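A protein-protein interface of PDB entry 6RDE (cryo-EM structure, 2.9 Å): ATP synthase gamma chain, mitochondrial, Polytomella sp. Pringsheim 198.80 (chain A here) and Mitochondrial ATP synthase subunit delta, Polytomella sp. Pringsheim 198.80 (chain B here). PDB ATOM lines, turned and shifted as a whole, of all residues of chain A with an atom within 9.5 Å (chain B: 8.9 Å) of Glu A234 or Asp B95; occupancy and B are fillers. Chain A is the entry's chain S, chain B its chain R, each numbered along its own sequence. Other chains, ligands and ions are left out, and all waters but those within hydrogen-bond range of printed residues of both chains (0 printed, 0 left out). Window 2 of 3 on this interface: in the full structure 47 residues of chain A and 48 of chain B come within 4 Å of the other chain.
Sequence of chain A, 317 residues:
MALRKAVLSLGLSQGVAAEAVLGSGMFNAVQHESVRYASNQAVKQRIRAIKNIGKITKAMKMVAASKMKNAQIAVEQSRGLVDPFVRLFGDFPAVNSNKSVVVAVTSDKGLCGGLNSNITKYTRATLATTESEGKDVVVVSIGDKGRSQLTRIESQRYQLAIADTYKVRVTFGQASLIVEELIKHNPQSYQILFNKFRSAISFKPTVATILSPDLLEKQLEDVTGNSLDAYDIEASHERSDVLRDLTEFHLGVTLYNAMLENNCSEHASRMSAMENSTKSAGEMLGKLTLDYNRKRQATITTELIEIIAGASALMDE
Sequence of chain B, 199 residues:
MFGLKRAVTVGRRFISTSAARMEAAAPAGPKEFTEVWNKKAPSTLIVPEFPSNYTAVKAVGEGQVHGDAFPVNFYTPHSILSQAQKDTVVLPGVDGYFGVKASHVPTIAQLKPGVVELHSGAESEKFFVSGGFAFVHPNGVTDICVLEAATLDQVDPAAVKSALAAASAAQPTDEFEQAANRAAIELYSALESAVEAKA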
ATOM      1  N   TYR A 231       0.276 -23.321  17.832  1.00  0.00           N
ATOM      2  CA  TYR A 231       0.932 -22.685  18.962  1.00  0.00           C
ATOM      3  C   TYR A 231       2.345 -23.205  19.114  1.00  0.00           C
ATOM      4  O   TYR A 231       2.575 -24.415  19.071  1.00  0.00           O
ATOM      5  CB  TYR A 231       0.157 -22.955  20.241  1.00  0.00           C
ATOM      6  CG  TYR A 231      -1.237 -22.417  20.244  1.00  0.00           C
ATOM      7  CD1 TYR A 231      -1.493 -21.117  20.636  1.00  0.00           C
ATOM      8  CD2 TYR A 231      -2.300 -23.214  19.866  1.00  0.00           C
ATOM      9  CE1 TYR A 231      -2.763 -20.629  20.648  1.00  0.00           C
ATOM     10  CE2 TYR A 231      -3.578 -22.733  19.875  1.00  0.00           C
ATOM     11  CZ  TYR A 231      -3.803 -21.441  20.264  1.00  0.00           C
ATOM     12  OH  TYR A 231      -5.087 -20.966  20.274  1.00  0.00           O
ATOM     13  N   ASP A 232       3.290 -22.299  19.316  1.00  0.00           N
ATOM     14  CA  ASP A 232       4.677 -22.685  19.517  1.00  0.00           C
ATOM     15  C   ASP A 232       5.003 -22.688  21.001  1.00  0.00           C
ATOM     16  O   ASP A 232       5.111 -21.632  21.626  1.00  0.00           O
ATOM     17  CB  ASP A 232       5.603 -21.782  18.720  1.00  0.00           C
ATOM     18  CG  ASP A 232       5.612 -22.163  17.270  1.00  0.00           C
ATOM     19  OD1 ASP A 232       6.169 -23.235  16.975  1.00  0.00           O
ATOM     20  OD2 ASP A 232       5.054 -21.426  16.435  1.00  0.00           O
ATOM     21  N   ILE A 233       5.182 -23.889  21.542  1.00  0.00           N
ATOM     22  CA  ILE A 233       5.289 -24.113  22.975  1.00  0.00           C
ATOM     23  C   ILE A 233       6.622 -23.584  23.479  1.00  0.00           C
ATOM     24  O   ILE A 233       7.690 -24.052  23.073  1.00  0.00           O
ATOM     25  CB  ILE A 233       5.138 -25.602  23.296  1.00  0.00           C
ATOM     26  CG1 ILE A 233       3.782 -26.126  22.828  1.00  0.00           C
ATOM     27  CG2 ILE A 233       5.349 -25.837  24.755  1.00  0.00           C
ATOM     28  CD1 ILE A 233       2.607 -25.403  23.409  1.00  0.00           C
ATOM     29  N   GLU A 234       6.563 -22.615  24.384  1.00  0.00           N
ATOM     30  CA  GLU A 234       7.739 -22.022  25.007  1.00  0.00           C
ATOM     31  C   GLU A 234       7.902 -22.559  26.423  1.00  0.00           C
ATOM     32  O   GLU A 234       8.178 -21.831  27.369  1.00  0.00           O
ATOM     33  CB  GLU A 234       7.606 -20.497  24.965  1.00  0.00           C
ATOM     34  CG  GLU A 234       8.878 -19.631  25.077  1.00  0.00           C
ATOM     35  CD  GLU A 234       9.154 -19.122  26.475  1.00  0.00           C
ATOM     36  OE1 GLU A 234       8.200 -18.954  27.246  1.00  0.00           O
ATOM     37  OE2 GLU A 234      10.320 -18.881  26.812  1.00  0.00           O
ATOM     38  N   ALA A 235       7.679 -23.852  26.608  1.00  0.00           N
ATOM     39  CA  ALA A 235       7.869 -24.465  27.910  1.00  0.00           C
ATOM     40  C   ALA A 235       9.297 -24.972  28.046  1.00  0.00           C
ATOM     41  O   ALA A 235      10.094 -24.915  27.112  1.00  0.00           O
ATOM     42  CB  ALA A 235       6.873 -25.598  28.122  1.00  0.00           C
ATOM     43  N   SER A 236       9.627 -25.471  29.231  1.00  0.00           N
ATOM     44  CA  SER A 236      10.915 -26.120  29.433  1.00  0.00           C
ATOM     45  C   SER A 236      10.892 -27.557  28.944  1.00  0.00           C
ATOM     46  O   SER A 236      11.895 -28.053  28.425  1.00  0.00           O
ATOM     47  CB  SER A 236      11.309 -26.079  30.909  1.00  0.00           C
ATOM     48  OG  SER A 236      10.260 -26.553  31.728  1.00  0.00           O
ATOM     49  N   HIS A 237       9.767 -28.232  29.095  1.00  0.00           N
ATOM     50  CA  HIS A 237       9.603 -29.590  28.624  1.00  0.00           C
ATOM     51  C   HIS A 237       8.583 -29.602  27.491  1.00  0.00           C
ATOM     52  O   HIS A 237       8.115 -28.554  27.042  1.00  0.00           O
ATOM     53  CB  HIS A 237       9.243 -30.481  29.804  1.00  0.00           C
ATOM     54  CG  HIS A 237      10.328 -30.557  30.832  1.00  0.00           C
ATOM     55  ND1 HIS A 237      10.633 -29.508  31.671  1.00  0.00           N
ATOM     56  CD2 HIS A 237      11.193 -31.549  31.144  1.00  0.00           C
ATOM     57  CE1 HIS A 237      11.631 -29.855  32.463  1.00  0.00           C
ATOM     58  NE2 HIS A 237      11.989 -31.087  32.164  1.00  0.00           N
ATOM     59  N   GLU A 238       8.255 -30.788  26.991  1.00  0.00           N
ATOM     60  CA  GLU A 238       7.501 -30.860  25.748  1.00  0.00           C
ATOM     61  C   GLU A 238       6.003 -30.691  26.014  1.00  0.00           C
ATOM     62  O   GLU A 238       5.565 -30.467  27.143  1.00  0.00           O
ATOM     63  CB  GLU A 238       7.852 -32.146  24.999  1.00  0.00           C
ATOM     64  CG  GLU A 238       7.553 -33.438  25.712  1.00  0.00           C
ATOM     65  CD  GLU A 238       6.214 -34.017  25.320  1.00  0.00           C
ATOM     66  OE1 GLU A 238       5.685 -33.615  24.264  1.00  0.00           O
ATOM     67  OE2 GLU A 238       5.706 -34.889  26.055  1.00  0.00           O
ATOM     68  N   ARG A 239       5.221 -30.787  24.934  1.00  0.00           N
ATOM     69  CA  ARG A 239       3.847 -30.289  24.916  1.00  0.00           C
ATOM     70  C   ARG A 239       2.914 -31.067  25.837  1.00  0.00           C
ATOM     71  O   ARG A 239       1.955 -30.494  26.364  1.00  0.00           O
ATOM     72  CB  ARG A 239       3.315 -30.302  23.483  1.00  0.00           C
ATOM     73  CG  ARG A 239       2.021 -29.541  23.304  1.00  0.00           C
ATOM     74  CD  ARG A 239       1.684 -29.296  21.851  1.00  0.00           C
ATOM     75  NE  ARG A 239       0.934 -30.375  21.232  1.00  0.00           N
ATOM     76  CZ  ARG A 239       0.721 -30.447  19.927  1.00  0.00           C
ATOM     77  NH1 ARG A 239       1.198 -29.499  19.137  1.00  0.00           N
ATOM     78  NH2 ARG A 239       0.029 -31.449  19.408  1.00  0.00           N
ATOM     79  N   VAL A 242       3.355 -29.466  29.273  1.00  0.00           N
ATOM     80  CA  VAL A 242       2.807 -28.126  29.429  1.00  0.00           C
ATOM     81  C   VAL A 242       1.289 -28.189  29.391  1.00  0.00           C
ATOM     82  O   VAL A 242       0.620 -27.352  29.994  1.00  0.00           O
ATOM     83  CB  VAL A 242       3.390 -27.158  28.373  1.00  0.00           C
ATOM     84  CG1 VAL A 242       2.828 -27.390  27.006  1.00  0.00           C
ATOM     85  CG2 VAL A 242       3.165 -25.730  28.759  1.00  0.00           C
ATOM     86  N   LEU B  91       7.161 -10.533  28.327  1.00  0.00           N
ATOM     87  CA  LEU B  91       6.789 -11.594  29.244  1.00  0.00           C
ATOM     88  C   LEU B  91       7.999 -12.413  29.666  1.00  0.00           C
ATOM     89  O   LEU B  91       8.840 -12.750  28.828  1.00  0.00           O
ATOM     90  CB  LEU B  91       5.765 -12.519  28.599  1.00  0.00           C
ATOM     91  CG  LEU B  91       4.442 -11.849  28.305  1.00  0.00           C
ATOM     92  CD1 LEU B  91       3.797 -12.447  27.084  1.00  0.00           C
ATOM     93  CD2 LEU B  91       3.576 -12.026  29.506  1.00  0.00           C
ATOM     94  N   PRO B  92       8.114 -12.747  30.937  1.00  0.00           N
ATOM     95  CA  PRO B  92       9.261 -13.523  31.438  1.00  0.00           C
ATOM     96  C   PRO B  92       9.128 -15.038  31.300  1.00  0.00           C
ATOM     97  O   PRO B  92       8.808 -15.761  32.238  1.00  0.00           O
ATOM     98  CB  PRO B  92       9.318 -13.109  32.907  1.00  0.00           C
ATOM     99  CG  PRO B  92       7.926 -12.803  33.251  1.00  0.00           C
ATOM    100  CD  PRO B  92       7.280 -12.242  32.034  1.00  0.00           C
ATOM    101  N   GLY B  93       9.406 -15.536  30.099  1.00  0.00           N
ATOM    102  CA  GLY B  93       9.292 -16.953  29.825  1.00  0.00           C
ATOM    103  C   GLY B  93      10.339 -17.778  30.542  1.00  0.00           C
ATOM    104  O   GLY B  93      11.294 -17.268  31.123  1.00  0.00           O
ATOM    105  N   VAL B  94      10.147 -19.097  30.508  1.00  0.00           N
ATOM    106  CA  VAL B  94      11.107 -19.981  31.147  1.00  0.00           C
ATOM    107  C   VAL B  94      12.388 -20.104  30.332  1.00  0.00           C
ATOM    108  O   VAL B  94      13.405 -20.573  30.849  1.00  0.00           O
ATOM    109  CB  VAL B  94      10.487 -21.362  31.399  1.00  0.00           C
ATOM    110  CG1 VAL B  94       9.394 -21.262  32.426  1.00  0.00           C
ATOM    111  CG2 VAL B  94       9.952 -21.920  30.128  1.00  0.00           C
ATOM    112  N   ASP B  95      12.369 -19.706  29.064  1.00  0.00           N
ATOM    113  CA  ASP B  95      13.601 -19.548  28.312  1.00  0.00           C
ATOM    114  C   ASP B  95      14.169 -18.143  28.428  1.00  0.00           C
ATOM    115  O   ASP B  95      15.336 -17.932  28.088  1.00  0.00           O
ATOM    116  CB  ASP B  95      13.374 -19.885  26.837  1.00  0.00           C
ATOM    117  CG  ASP B  95      12.927 -21.318  26.627  1.00  0.00           C
ATOM    118  OD1 ASP B  95      13.265 -22.181  27.463  1.00  0.00           O
ATOM    119  OD2 ASP B  95      12.239 -21.584  25.622  1.00  0.00           O
ATOM    120  N   GLY B  96      13.380 -17.191  28.887  1.00  0.00           N
ATOM    121  CA  GLY B  96      13.850 -15.835  29.092  1.00  0.00           C
ATOM    122  C   GLY B  96      12.802 -14.836  28.650  1.00  0.00           C
ATOM    123  O   GLY B  96      11.779 -15.190  28.076  1.00  0.00           O
ATOM    124  N   TYR B  97      13.094 -13.567  28.924  1.00  0.00           N
ATOM    125  CA  TYR B  97      12.167 -12.469  28.660  1.00  0.00           C
ATOM    126  C   TYR B  97      11.974 -12.298  27.164  1.00  0.00           C
ATOM    127  O   TYR B  97      12.850 -11.769  26.480  1.00  0.00           O
ATOM    128  CB  TYR B  97      12.700 -11.171  29.253  1.00  0.00           C
ATOM    129  CG  TYR B  97      12.533 -11.003  30.737  1.00  0.00           C
ATOM    130  CD1 TYR B  97      13.344 -11.687  31.629  1.00  0.00           C
ATOM    131  CD2 TYR B  97      11.589 -10.129  31.248  1.00  0.00           C
ATOM    132  CE1 TYR B  97      13.203 -11.524  32.985  1.00  0.00           C
ATOM    133  CE2 TYR B  97      11.442  -9.957  32.606  1.00  0.00           C
ATOM    134  CZ  TYR B  97      12.251 -10.657  33.469  1.00  0.00           C
ATOM    135  OH  TYR B  97      12.106 -10.490  34.826  1.00  0.00           O
ATOM    136  N   PHE B  98      10.830 -12.712  26.646  1.00  0.00           N
ATOM    137  CA  PHE B  98      10.535 -12.470  25.246  1.00  0.00           C
ATOM    138  C   PHE B  98       9.622 -11.263  25.122  1.00  0.00           C
ATOM    139  O   PHE B  98       9.168 -10.697  26.115  1.00  0.00           O
ATOM    140  CB  PHE B  98       9.926 -13.707  24.568  1.00  0.00           C
ATOM    141  CG  PHE B  98       8.646 -14.195  25.173  1.00  0.00           C
ATOM    142  CD1 PHE B  98       8.657 -15.091  26.225  1.00  0.00           C
ATOM    143  CD2 PHE B  98       7.429 -13.811  24.645  1.00  0.00           C
ATOM    144  CE1 PHE B  98       7.482 -15.558  26.760  1.00  0.00           C
ATOM    145  CE2 PHE B  98       6.256 -14.280  25.176  1.00  0.00           C
ATOM    146  CZ  PHE B  98       6.284 -15.147  26.233  1.00  0.00           C
ATOM    147  N   GLY B  99       9.381 -10.854  23.886  1.00  0.00           N
ATOM    148  CA  GLY B  99       8.533  -9.710  23.642  1.00  0.00           C
ATOM    149  C   GLY B  99       7.508  -9.991  22.572  1.00  0.00           C
ATOM    150  O   GLY B  99       7.859 -10.417  21.473  1.00  0.00           O
ATOM    151  N   HIS B 104       2.450 -11.432  16.320  1.00  0.00           N
ATOM    152  CA  HIS B 104       3.334 -12.442  16.886  1.00  0.00           C
ATOM    153  C   HIS B 104       2.866 -13.839  16.501  1.00  0.00           C
ATOM    154  O   HIS B 104       1.722 -14.053  16.099  1.00  0.00           O
ATOM    155  CB  HIS B 104       3.365 -12.304  18.408  1.00  0.00           C
ATOM    156  CG  HIS B 104       4.568 -12.901  19.067  1.00  0.00           C
ATOM    157  ND1 HIS B 104       5.704 -12.173  19.339  1.00  0.00           N
ATOM    158  CD2 HIS B 104       4.791 -14.141  19.559  1.00  0.00           C
ATOM    159  CE1 HIS B 104       6.587 -12.946  19.946  1.00  0.00           C
ATOM    160  NE2 HIS B 104       6.058 -14.146  20.089  1.00  0.00           N
ATOM    161  N   VAL B 105       3.776 -14.797  16.618  1.00  0.00           N
ATOM    162  CA  VAL B 105       3.469 -16.196  16.337  1.00  0.00           C
ATOM    163  C   VAL B 105       2.568 -16.679  17.469  1.00  0.00           C
ATOM    164  O   VAL B 105       2.620 -16.112  18.569  1.00  0.00           O
ATOM    165  CB  VAL B 105       4.766 -17.017  16.179  1.00  0.00           C
ATOM    166  CG1 VAL B 105       5.461 -17.238  17.503  1.00  0.00           C
ATOM    167  CG2 VAL B 105       4.523 -18.321  15.468  1.00  0.00           C
ATOM    168  N   PRO B 106       1.657 -17.620  17.234  1.00  0.00           N
ATOM    169  CA  PRO B 106       0.925 -18.218  18.353  1.00  0.00           C
ATOM    170  C   PRO B 106       1.856 -18.948  19.307  1.00  0.00           C
ATOM    171  O   PRO B 106       2.677 -19.767  18.895  1.00  0.00           O
ATOM    172  CB  PRO B 106      -0.045 -19.174  17.663  1.00  0.00           C
ATOM    173  CG  PRO B 106      -0.302 -18.544  16.383  1.00  0.00           C
ATOM    174  CD  PRO B 106       0.960 -17.850  15.961  1.00  0.00           C
ATOM    175  N   THR B 107       1.723 -18.636  20.593  1.00  0.00           N
ATOM    176  CA  THR B 107       2.684 -19.061  21.602  1.00  0.00           C
ATOM    177  C   THR B 107       1.950 -19.385  22.892  1.00  0.00           C
ATOM    178  O   THR B 107       1.322 -18.502  23.478  1.00  0.00           O
ATOM    179  CB  THR B 107       3.714 -17.961  21.856  1.00  0.00           C
ATOM    180  OG1 THR B 107       4.347 -17.598  20.628  1.00  0.00           O
ATOM    181  CG2 THR B 107       4.761 -18.448  22.799  1.00  0.00           C
ATOM    182  N   ILE B 108       2.032 -20.631  23.342  1.00  0.00           N
ATOM    183  CA  ILE B 108       1.627 -21.008  24.692  1.00  0.00           C
ATOM    184  C   ILE B 108       2.904 -21.053  25.515  1.00  0.00           C
ATOM    185  O   ILE B 108       3.672 -22.012  25.442  1.00  0.00           O
ATOM    186  CB  ILE B 108       0.892 -22.347  24.726  1.00  0.00           C
ATOM    187  CG1 ILE B 108      -0.371 -22.284  23.881  1.00  0.00           C
ATOM    188  CG2 ILE B 108       0.537 -22.703  26.137  1.00  0.00           C
ATOM    189  CD1 ILE B 108      -1.036 -23.614  23.714  1.00  0.00           C
ATOM    190  N   ALA B 109       3.143 -20.012  26.291  1.00  0.00           N
ATOM    191  CA  ALA B 109       4.428 -19.807  26.936  1.00  0.00           C
ATOM    192  C   ALA B 109       4.269 -19.898  28.440  1.00  0.00           C
ATOM    193  O   ALA B 109       3.541 -19.101  29.035  1.00  0.00           O
ATOM    194  CB  ALA B 109       4.998 -18.451  26.554  1.00  0.00           C
ATOM    195  N   GLN B 110       4.946 -20.857  29.051  1.00  0.00           N
ATOM    196  CA  GLN B 110       5.046 -20.893  30.500  1.00  0.00           C
ATOM    197  C   GLN B 110       5.956 -19.768  30.953  1.00  0.00           C
ATOM    198  O   GLN B 110       6.943 -19.460  30.285  1.00  0.00           O
ATOM    199  CB  GLN B 110       5.583 -22.239  30.969  1.00  0.00           C
ATOM    200  CG  GLN B 110       5.529 -22.419  32.467  1.00  0.00           C
ATOM    201  CD  GLN B 110       5.692 -23.852  32.898  1.00  0.00           C
ATOM    202  OE1 GLN B 110       5.746 -24.758  32.070  1.00  0.00           O
ATOM    203  NE2 GLN B 110       5.772 -24.067  34.203  1.00  0.00           N
ATOM    204  N   LEU B 111       5.613 -19.128  32.060  1.00  0.00           N
ATOM    205  CA  LEU B 111       6.413 -18.040  32.586  1.00  0.00           C
ATOM    206  C   LEU B 111       6.962 -18.405  33.954  1.00  0.00           C
ATOM    207  O   LEU B 111       6.238 -18.921  34.807  1.00  0.00           O
ATOM    208  CB  LEU B 111       5.604 -16.751  32.687  1.00  0.00           C
ATOM    209  CG  LEU B 111       4.848 -16.222  31.473  1.00  0.00           C
ATOM    210  CD1 LEU B 111       4.219 -14.905  31.855  1.00  0.00           C
ATOM    211  CD2 LEU B 111       5.730 -16.061  30.278  1.00  0.00           C
ATOM    212  N   LYS B 112       8.240 -18.128  34.154  1.00  0.00           N
ATOM    213  CA  LYS B 112       8.877 -18.244  35.452  1.00  0.00           C
ATOM    214  C   LYS B 112       8.536 -16.998  36.258  1.00  0.00           C
ATOM    215  O   LYS B 112       7.915 -16.076  35.729  1.00  0.00           O
ATOM    216  CB  LYS B 112      10.381 -18.418  35.256  1.00  0.00           C
ATOM    217  CG  LYS B 112      11.082 -17.161  34.830  1.00  0.00           C
ATOM    218  CD  LYS B 112      12.542 -17.406  34.551  1.00  0.00           C
ATOM    219  CE  LYS B 112      13.270 -16.094  34.359  1.00  0.00           C
ATOM    220  NZ  LYS B 112      12.748 -15.345  33.189  1.00  0.00           N
ATOM    221  N   GLY B 132       3.092 -18.146  35.794  1.00  0.00           N
ATOM    222  CA  GLY B 132       1.861 -18.624  35.210  1.00  0.00           C
ATOM    223  C   GLY B 132       1.821 -18.232  33.757  1.00  0.00           C
ATOM    224  O   GLY B 132       2.449 -17.253  33.372  1.00  0.00           O
ATOM    225  N   PHE B 133       1.030 -18.932  32.964  1.00  0.00           N
ATOM    226  CA  PHE B 133       1.193 -19.011  31.524  1.00  0.00           C
ATOM    227  C   PHE B 133       0.790 -17.721  30.819  1.00  0.00           C
ATOM    228  O   PHE B 133       0.152 -16.839  31.385  1.00  0.00           O
ATOM    229  CB  PHE B 133       0.383 -20.175  30.984  1.00  0.00           C
ATOM    230  CG  PHE B 133       0.827 -21.492  31.508  1.00  0.00           C
ATOM    231  CD1 PHE B 133       1.743 -22.236  30.807  1.00  0.00           C
ATOM    232  CD2 PHE B 133       0.340 -21.992  32.704  1.00  0.00           C
ATOM    233  CE1 PHE B 133       2.165 -23.442  31.283  1.00  0.00           C
ATOM    234  CE2 PHE B 133       0.754 -23.203  33.166  1.00  0.00           C
ATOM    235  CZ  PHE B 133       1.671 -23.924  32.459  1.00  0.00           C
ATOM    236  N   ALA B 134       1.189 -17.631  29.554  1.00  0.00           N
ATOM    237  CA  ALA B 134       0.834 -16.526  28.675  1.00  0.00           C
ATOM    238  C   ALA B 134       0.547 -17.103  27.303  1.00  0.00           C
ATOM    239  O   ALA B 134       1.359 -17.862  26.774  1.00  0.00           O
ATOM    240  CB  ALA B 134       1.953 -15.492  28.596  1.00  0.00           C
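The backbone NH (N) of Asp B95 lies within hydrogen-bond range of the side-chain carboxylate (OE2) of Glu A234 (3.2 Å). The backbone NH of Asp A232 is in hydrogen-bond range of the backbone carbonyl oxygen of Pro B106 (2.6 Å). N of Glu A234 sits at hydrogen-bond distance from O of Ile B108 (3.1 Å). OE1 of Glu A234 sits close to O of Gln B110 (3.3 Å).
O of Leu B91 is in hydrogen-bond range of N of Phe B98, 3.0 Å away. The backbone carbonyl oxygen of Gly B93 is in hydrogen-bond range of the side-chain amino group of Lys B112 (3.2 Å). N of Val B94 lies within hydrogen-bond range of O of Gln B110 (3.2 Å). O of Val B105 is in hydrogen-bond range of OG1 of Thr B107 (3.1 Å). The backbone carbonyl oxygen (O) of Ala B109 is in hydrogen-bond range of the backbone NH (N) of Ala B134 (2.8 Å). ND1 of His A237 is in hydrogen-bond range of OG of Ser A236.
Pro B106 touches Tyr A231. CG2 of Val B105 touches OD2 of Asp A232, at 3.3 Å. CG2 of Thr B107 touches O of Asp A232, at 3.4 Å. Ile A233 touches Ile B108. OE1 of Glu A234 touches CA of Gly B93 (3.4 Å). CG2 of Val B94 touches O of Glu A234, at 3.3 Å. Phe B98 touches Glu A234 (CE1 to OE1, 3.5 Å). Glu A234 touches Ala B109 (OE1 to CB, 3.3 Å). Ser A236 touches Val B94 (N to CG2, 3.7 Å). Val A242 touches Phe B133.
Glu A234 touches just these residues of chain B: Gly B93, Val B94, Asp B95, Phe B98, Ile B108, Ala B109 and Gln B110. Asp B95 touches just one residue of chain A: Glu A234 (3.2 Å). Of chain B, only Val B94 (3.8 Å) comes within 4 Å of Ala A235. Gly B93 touches just one residue of chain A: Glu A234 (3.4 Å). Val B94 touches just these residues of chain A: Glu A234 (3.3 Å), Ala A235 (3.8 Å) and Ser A236 (3.7 Å). Ala B109 touches just one residue of chain A: Glu A234. Of the printed residues of chain A, Pro B106 touches Tyr A231 (3.4 Å) and Asp A232 (2.6 Å). Printed residues of chain B within 4 Å of Ser A236: Val B94 (3.7 Å). Arg A239 touches none of the printed residues of chain B. Leu B91 touches none of the printed residues of chain A.
Hydrophobic or aromatic side chains of chain B within 4 Å of the printed part of chain A: Val B94, Phe B98, Val B105, Pro B106, Ile B108, Ala B109 and Phe B133. Of the 10 printed residues of chain A, 7 touch a printed residue of chain B. Hydrophobic or aromatic side chains of chain A within 4 Å of the printed part of chain B: Tyr A231, Ile A233 and Val A242. Among the printed residues, no Asp or Glu carboxylate lies within 4 Å of a Lys or Arg side-chain nitrogen of the other chain.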
